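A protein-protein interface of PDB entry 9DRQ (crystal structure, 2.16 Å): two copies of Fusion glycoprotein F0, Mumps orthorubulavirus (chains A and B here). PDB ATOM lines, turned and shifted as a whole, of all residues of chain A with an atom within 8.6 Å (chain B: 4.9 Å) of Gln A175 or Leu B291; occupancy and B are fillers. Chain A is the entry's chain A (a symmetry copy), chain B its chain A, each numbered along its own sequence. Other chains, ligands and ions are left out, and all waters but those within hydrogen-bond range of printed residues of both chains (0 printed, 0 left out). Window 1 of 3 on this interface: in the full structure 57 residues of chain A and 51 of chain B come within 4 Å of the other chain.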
ATOM      1  N   PRO A  63     -18.086  12.708  28.141  1.00  0.00           N
ATOM      2  CA  PRO A  63     -18.677  12.960  26.809  1.00  0.00           C
ATOM      3  C   PRO A  63     -17.873  12.386  25.650  1.00  0.00           C
ATOM      4  O   PRO A  63     -18.475  11.946  24.663  1.00  0.00           O
ATOM      5  CB  PRO A  63     -18.740  14.493  26.735  1.00  0.00           C
ATOM      6  CG  PRO A  63     -18.812  14.937  28.154  1.00  0.00           C
ATOM      7  CD  PRO A  63     -17.937  13.955  28.915  1.00  0.00           C
ATOM      8  N   THR A 170      -7.963  22.485  28.419  1.00  0.00           N
ATOM      9  CA  THR A 170      -8.023  22.950  27.042  1.00  0.00           C
ATOM     10  C   THR A 170      -8.387  21.819  26.079  1.00  0.00           C
ATOM     11  O   THR A 170      -8.918  22.085  25.003  1.00  0.00           O
ATOM     12  CB  THR A 170      -6.684  23.609  26.660  1.00  0.00           C
ATOM     13  OG1 THR A 170      -6.810  24.302  25.408  1.00  0.00           O
ATOM     14  CG2 THR A 170      -5.575  22.580  26.560  1.00  0.00           C
ATOM     15  N   CYS A 171      -8.156  20.564  26.462  1.00  0.00           N
ATOM     16  CA  CYS A 171      -8.523  19.428  25.631  1.00  0.00           C
ATOM     17  C   CYS A 171     -10.028  19.208  25.532  1.00  0.00           C
ATOM     18  O   CYS A 171     -10.482  18.558  24.584  1.00  0.00           O
ATOM     19  CB  CYS A 171      -7.873  18.150  26.174  1.00  0.00           C
ATOM     20  SG  CYS A 171      -6.092  18.111  25.943  1.00  0.00           S
ATOM     21  N   PHE A 172     -10.816  19.702  26.479  1.00  0.00           N
ATOM     22  CA  PHE A 172     -12.228  19.353  26.534  1.00  0.00           C
ATOM     23  C   PHE A 172     -13.063  20.529  26.062  1.00  0.00           C
ATOM     24  O   PHE A 172     -12.912  21.648  26.563  1.00  0.00           O
ATOM     25  CB  PHE A 172     -12.633  18.905  27.935  1.00  0.00           C
ATOM     26  CG  PHE A 172     -11.807  17.762  28.440  1.00  0.00           C
ATOM     27  CD1 PHE A 172     -12.047  16.468  27.999  1.00  0.00           C
ATOM     28  CD2 PHE A 172     -10.743  17.990  29.311  1.00  0.00           C
ATOM     29  CE1 PHE A 172     -11.269  15.429  28.448  1.00  0.00           C
ATOM     30  CE2 PHE A 172      -9.962  16.951  29.755  1.00  0.00           C
ATOM     31  CZ  PHE A 172     -10.223  15.676  29.328  1.00  0.00           C
ATOM     32  N   GLN A 173     -13.933  20.266  25.090  1.00  0.00           N
ATOM     33  CA  GLN A 173     -14.800  21.268  24.480  1.00  0.00           C
ATOM     34  C   GLN A 173     -16.218  20.767  24.679  1.00  0.00           C
ATOM     35  O   GLN A 173     -16.758  20.035  23.832  1.00  0.00           O
ATOM     36  CB  GLN A 173     -14.469  21.470  23.002  1.00  0.00           C
ATOM     37  CG  GLN A 173     -13.211  22.288  22.766  1.00  0.00           C
ATOM     38  CD  GLN A 173     -12.385  21.758  21.611  1.00  0.00           C
ATOM     39  OE1 GLN A 173     -12.342  20.547  21.371  1.00  0.00           O
ATOM     40  NE2 GLN A 173     -11.726  22.659  20.888  1.00  0.00           N
ATOM     41  N   PRO A 174     -16.860  21.131  25.787  1.00  0.00           N
ATOM     42  CA  PRO A 174     -18.199  20.595  26.070  1.00  0.00           C
ATOM     43  C   PRO A 174     -19.271  21.111  25.128  1.00  0.00           C
ATOM     44  O   PRO A 174     -20.386  20.574  25.136  1.00  0.00           O
ATOM     45  CB  PRO A 174     -18.455  21.045  27.514  1.00  0.00           C
ATOM     46  CG  PRO A 174     -17.598  22.275  27.688  1.00  0.00           C
ATOM     47  CD  PRO A 174     -16.403  22.099  26.804  1.00  0.00           C
ATOM     48  N   GLN A 175     -18.983  22.133  24.315  1.00  0.00           N
ATOM     49  CA  GLN A 175     -20.012  22.645  23.419  1.00  0.00           C
ATOM     50  C   GLN A 175     -20.252  21.728  22.230  1.00  0.00           C
ATOM     51  O   GLN A 175     -21.309  21.828  21.593  1.00  0.00           O
ATOM     52  CB  GLN A 175     -19.649  24.042  22.913  1.00  0.00           C
ATOM     53  CG  GLN A 175     -18.690  24.049  21.735  1.00  0.00           C
ATOM     54  CD  GLN A 175     -17.243  23.864  22.161  1.00  0.00           C
ATOM     55  OE1 GLN A 175     -16.946  23.671  23.347  1.00  0.00           O
ATOM     56  NE2 GLN A 175     -16.331  23.933  21.192  1.00  0.00           N
ATOM     57  N   LEU A 176     -19.302  20.844  21.917  1.00  0.00           N
ATOM     58  CA  LEU A 176     -19.408  20.004  20.729  1.00  0.00           C
ATOM     59  C   LEU A 176     -20.406  18.881  20.966  1.00  0.00           C
ATOM     60  O   LEU A 176     -20.427  18.263  22.032  1.00  0.00           O
ATOM     61  CB  LEU A 176     -18.045  19.411  20.356  1.00  0.00           C
ATOM     62  CG  LEU A 176     -16.925  20.378  19.958  1.00  0.00           C
ATOM     63  CD1 LEU A 176     -15.619  19.648  19.793  1.00  0.00           C
ATOM     64  CD2 LEU A 176     -17.287  21.108  18.667  1.00  0.00           C
ATOM     65  N   THR A 177     -21.237  18.618  19.960  1.00  0.00           N
ATOM     66  CA  THR A 177     -22.115  17.452  20.009  1.00  0.00           C
ATOM     67  C   THR A 177     -21.361  16.157  19.747  1.00  0.00           C
ATOM     68  O   THR A 177     -21.742  15.110  20.279  1.00  0.00           O
ATOM     69  CB  THR A 177     -23.242  17.586  18.982  1.00  0.00           C
ATOM     70  OG1 THR A 177     -22.677  17.921  17.713  1.00  0.00           O
ATOM     71  CG2 THR A 177     -24.203  18.669  19.395  1.00  0.00           C
ATOM     72  N   ASN A 178     -20.327  16.199  18.903  1.00  0.00           N
ATOM     73  CA  ASN A 178     -19.482  15.043  18.610  1.00  0.00           C
ATOM     74  C   ASN A 178     -18.056  15.362  19.048  1.00  0.00           C
ATOM     75  O   ASN A 178     -17.149  15.447  18.209  1.00  0.00           O
ATOM     76  CB  ASN A 178     -19.519  14.670  17.127  1.00  0.00           C
ATOM     77  CG  ASN A 178     -20.786  13.917  16.742  1.00  0.00           C
ATOM     78  OD1 ASN A 178     -21.007  12.790  17.185  1.00  0.00           O
ATOM     79  ND2 ASN A 178     -21.621  14.532  15.907  1.00  0.00           N
ATOM     80  N   PRO A 179     -17.817  15.522  20.364  1.00  0.00           N
ATOM     81  CA  PRO A 179     -16.479  15.949  20.811  1.00  0.00           C
ATOM     82  C   PRO A 179     -15.364  15.049  20.335  1.00  0.00           C
ATOM     83  O   PRO A 179     -14.273  15.549  20.049  1.00  0.00           O
ATOM     84  CB  PRO A 179     -16.598  15.939  22.339  1.00  0.00           C
ATOM     85  CG  PRO A 179     -17.730  15.003  22.616  1.00  0.00           C
ATOM     86  CD  PRO A 179     -18.702  15.248  21.502  1.00  0.00           C
ATOM     87  N   SER A 182     -13.709  16.018  16.704  1.00  0.00           N
ATOM     88  CA  SER A 182     -12.851  17.155  16.450  1.00  0.00           C
ATOM     89  C   SER A 182     -11.399  16.719  16.602  1.00  0.00           C
ATOM     90  O   SER A 182     -11.094  15.864  17.437  1.00  0.00           O
ATOM     91  CB  SER A 182     -13.158  18.295  17.411  1.00  0.00           C
ATOM     92  OG  SER A 182     -12.144  18.401  18.398  1.00  0.00           O
ATOM     93  N   ARG B  17     -28.983  26.184  21.235  1.00  0.00           N
ATOM     94  CA  ARG B  17     -28.582  26.437  22.610  1.00  0.00           C
ATOM     95  C   ARG B  17     -29.441  27.544  23.193  1.00  0.00           C
ATOM     96  O   ARG B  17     -29.923  28.423  22.475  1.00  0.00           O
ATOM     97  CB  ARG B  17     -27.103  26.828  22.715  1.00  0.00           C
ATOM     98  CG  ARG B  17     -26.150  25.730  22.262  1.00  0.00           C
ATOM     99  CD  ARG B  17     -24.693  26.147  22.362  1.00  0.00           C
ATOM    100  NE  ARG B  17     -23.819  25.084  21.886  1.00  0.00           N
ATOM    101  CZ  ARG B  17     -23.385  24.993  20.629  1.00  0.00           C
ATOM    102  NH1 ARG B  17     -23.745  25.913  19.733  1.00  0.00           N
ATOM    103  NH2 ARG B  17     -22.600  23.987  20.262  1.00  0.00           N
ATOM    104  N   ALA B 217     -15.377  24.872  30.140  1.00  0.00           N
ATOM    105  CA  ALA B 217     -15.909  25.987  29.373  1.00  0.00           C
ATOM    106  C   ALA B 217     -15.486  27.338  29.924  1.00  0.00           C
ATOM    107  O   ALA B 217     -15.897  28.362  29.378  1.00  0.00           O
ATOM    108  CB  ALA B 217     -17.439  25.910  29.320  1.00  0.00           C
ATOM    109  N   ARG B 273     -24.492  31.709  12.880  1.00  0.00           N
ATOM    110  CA  ARG B 273     -25.055  31.570  14.212  1.00  0.00           C
ATOM    111  C   ARG B 273     -26.115  32.638  14.386  1.00  0.00           C
ATOM    112  O   ARG B 273     -25.821  33.831  14.264  1.00  0.00           O
ATOM    113  CB  ARG B 273     -23.965  31.673  15.291  1.00  0.00           C
ATOM    114  CG  ARG B 273     -24.478  31.452  16.694  1.00  0.00           C
ATOM    115  CD  ARG B 273     -23.297  31.278  17.691  1.00  0.00           C
ATOM    116  NE  ARG B 273     -22.687  29.947  17.651  1.00  0.00           N
ATOM    117  CZ  ARG B 273     -21.427  29.664  18.002  1.00  0.00           C
ATOM    118  NH1 ARG B 273     -20.585  30.613  18.408  1.00  0.00           N
ATOM    119  NH2 ARG B 273     -21.003  28.413  17.948  1.00  0.00           N
ATOM    120  N   ALA B 286     -21.445  35.408  19.215  1.00  0.00           N
ATOM    121  CA  ALA B 286     -21.092  34.857  20.535  1.00  0.00           C
ATOM    122  C   ALA B 286     -19.592  34.592  20.656  1.00  0.00           C
ATOM    123  O   ALA B 286     -19.165  33.636  21.309  1.00  0.00           O
ATOM    124  CB  ALA B 286     -21.879  33.582  20.832  1.00  0.00           C
ATOM    125  N   CYS B 289     -18.550  34.859  24.228  1.00  0.00           N
ATOM    126  CA  CYS B 289     -19.360  34.130  25.197  1.00  0.00           C
ATOM    127  C   CYS B 289     -18.767  32.748  25.450  1.00  0.00           C
ATOM    128  O   CYS B 289     -17.845  32.300  24.767  1.00  0.00           O
ATOM    129  CB  CYS B 289     -20.816  34.015  24.728  1.00  0.00           C
ATOM    130  SG  CYS B 289     -21.620  35.608  24.356  1.00  0.00           S
ATOM    131  N   LYS B 290     -19.311  32.078  26.458  1.00  0.00           N
ATOM    132  CA  LYS B 290     -18.944  30.715  26.799  1.00  0.00           C
ATOM    133  C   LYS B 290     -20.062  29.762  26.404  1.00  0.00           C
ATOM    134  O   LYS B 290     -21.250  30.076  26.561  1.00  0.00           O
ATOM    135  CB  LYS B 290     -18.645  30.580  28.290  1.00  0.00           C
ATOM    136  CG  LYS B 290     -17.438  31.393  28.728  1.00  0.00           C
ATOM    137  CD  LYS B 290     -17.898  32.577  29.541  1.00  0.00           C
ATOM    138  CE  LYS B 290     -16.742  33.165  30.346  1.00  0.00           C
ATOM    139  NZ  LYS B 290     -15.520  33.240  29.510  1.00  0.00           N
ATOM    140  N   LEU B 291     -19.669  28.596  25.894  1.00  0.00           N
ATOM    141  CA  LEU B 291     -20.601  27.647  25.313  1.00  0.00           C
ATOM    142  C   LEU B 291     -20.468  26.291  25.989  1.00  0.00           C
ATOM    143  O   LEU B 291     -19.354  25.794  26.192  1.00  0.00           O
ATOM    144  CB  LEU B 291     -20.368  27.515  23.807  1.00  0.00           C
ATOM    145  CG  LEU B 291     -20.798  28.701  22.928  1.00  0.00           C
ATOM    146  CD1 LEU B 291     -19.772  29.821  22.964  1.00  0.00           C
ATOM    147  CD2 LEU B 291     -21.029  28.232  21.497  1.00  0.00           C
ATOM    148  N   THR B 292     -21.603  25.707  26.349  1.00  0.00           N
ATOM    149  CA  THR B 292     -21.714  24.284  26.612  1.00  0.00           C
ATOM    150  C   THR B 292     -22.586  23.674  25.518  1.00  0.00           C
ATOM    151  O   THR B 292     -22.982  24.356  24.561  1.00  0.00           O
ATOM    152  CB  THR B 292     -22.286  24.018  28.001  1.00  0.00           C
ATOM    153  OG1 THR B 292     -23.641  24.473  28.049  1.00  0.00           O
ATOM    154  CG2 THR B 292     -21.462  24.727  29.080  1.00  0.00           C
ATOM    155  N   ARG B 293     -22.891  22.381  25.662  1.00  0.00           N
ATOM    156  CA  ARG B 293     -23.615  21.688  24.602  1.00  0.00           C
ATOM    157  C   ARG B 293     -24.982  22.312  24.381  1.00  0.00           C
ATOM    158  O   ARG B 293     -25.428  22.467  23.242  1.00  0.00           O
ATOM    159  CB  ARG B 293     -23.759  20.191  24.918  1.00  0.00           C
ATOM    160  CG  ARG B 293     -24.214  19.386  23.689  1.00  0.00           C
ATOM    161  CD  ARG B 293     -24.201  17.874  23.882  1.00  0.00           C
ATOM    162  NE  ARG B 293     -22.852  17.339  24.067  1.00  0.00           N
ATOM    163  CZ  ARG B 293     -22.572  16.040  24.150  1.00  0.00           C
ATOM    164  NH1 ARG B 293     -21.321  15.630  24.327  1.00  0.00           N
ATOM    165  NH2 ARG B 293     -23.550  15.152  24.051  1.00  0.00           N
ATOM    166  N   HIS B 295     -26.083  25.342  26.049  1.00  0.00           N
ATOM    167  CA  HIS B 295     -26.224  26.684  26.589  1.00  0.00           C
ATOM    168  C   HIS B 295     -25.140  27.612  26.086  1.00  0.00           C
ATOM    169  O   HIS B 295     -24.002  27.203  25.844  1.00  0.00           O
ATOM    170  CB  HIS B 295     -26.194  26.670  28.118  1.00  0.00           C
ATOM    171  CG  HIS B 295     -27.460  26.167  28.712  1.00  0.00           C
ATOM    172  ND1 HIS B 295     -27.692  24.830  28.942  1.00  0.00           N
ATOM    173  CD2 HIS B 295     -28.592  26.814  29.066  1.00  0.00           C
ATOM    174  CE1 HIS B 295     -28.899  24.679  29.453  1.00  0.00           C
ATOM    175  NE2 HIS B 295     -29.468  25.867  29.532  1.00  0.00           N
ATOM    176  N   ILE B 296     -25.512  28.884  25.962  1.00  0.00           N
ATOM    177  CA  ILE B 296     -24.575  29.965  25.703  1.00  0.00           C
ATOM    178  C   ILE B 296     -24.715  30.977  26.821  1.00  0.00           C
ATOM    179  O   ILE B 296     -25.822  31.467  27.095  1.00  0.00           O
ATOM    180  CB  ILE B 296     -24.816  30.626  24.337  1.00  0.00           C
ATOM    181  CG1 ILE B 296     -24.714  29.580  23.242  1.00  0.00           C
ATOM    182  CG2 ILE B 296     -23.794  31.753  24.097  1.00  0.00           C
ATOM    183  CD1 ILE B 296     -24.605  30.178  21.854  1.00  0.00           C
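The guanidinium group (NH2) of Arg B17 lies within hydrogen-bond range of the backbone carbonyl oxygen (O) of Gln A175, 2.8 Å away.
The backbone NH (N) of Arg B293 lies within hydrogen-bond range of the backbone carbonyl oxygen (O) of Pro A174 (3.1 Å).
NE of Arg B293 lies within hydrogen-bond range of O of Leu A176.
The guanidinium group (NE) of Arg B17 is in hydrogen-bond range of the backbone carbonyl oxygen (O) of Thr B292.
The guanidinium group (NE) of Arg B17 is in hydrogen-bond range of the backbone carbonyl oxygen (O) of Arg B293 (3.4 Å).
The backbone NH (N) of His B295 is in hydrogen-bond range of the side-chain hydroxyl (OG1) of Thr B292.
Arg B293 touches Pro A63.
Pro A174 touches Ala B217 (CG to CB, 3.99 Å).
Pro A174 touches Thr B292 (O to C, 3.8 Å).
Gln A175 touches Leu B291.
Gln A175 touches Thr B292 (CA to C, 3.5 Å).
Arg B293 touches Gln A175.
Pro A179 touches Arg B293 (CD to NH1, 3.9 Å).
Gln A175 touches just these residues of chain B: Arg B17, Leu B291, Thr B292 and Arg B293.
Of chain A, only Gln A175 comes within 4 Å of Leu B291.
Thr B292 touches just these residues of chain A: Pro A174 (3.8 Å) and Gln A175 (3.5 Å).
Printed residues of chain B within 4 Å of Pro A174: Ala B217 (3.99 Å), Thr B292 (3.8 Å) and Arg B293 (3.1 Å).
Printed residues of chain B within 4 Å of Leu A176: Arg B293 (3.3 Å).
Of the printed residues of chain A, Arg B293 touches Pro A63, Pro A174, Gln A175, Leu A176 and Pro A179.
Printed residues of chain A within 4 Å of Arg B17: Gln A175 (2.8 Å).
The nearest printed residue of chain A that does not touch Ala B217 is Phe A172 (5.4 Å).
Hydrophobic or aromatic side chains of chain B within 4 Å of the printed part of chain A: Ala B217 and Leu B291.
Hydrophobic or aromatic side chains of chain A within 4 Å of the printed part of chain B: Pro A63, Pro A174 and Pro A179.
Along chain A the printed residues that touch a printed residue of chain B span positions 63 to 179.
Among the printed residues, 10 pairs touch across the chains.
Among the printed residues, no Asp or Glu carboxylate lies within 4 Å of a Lys or Arg side-chain nitrogen of the other chain.
No position is printed for both chains.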
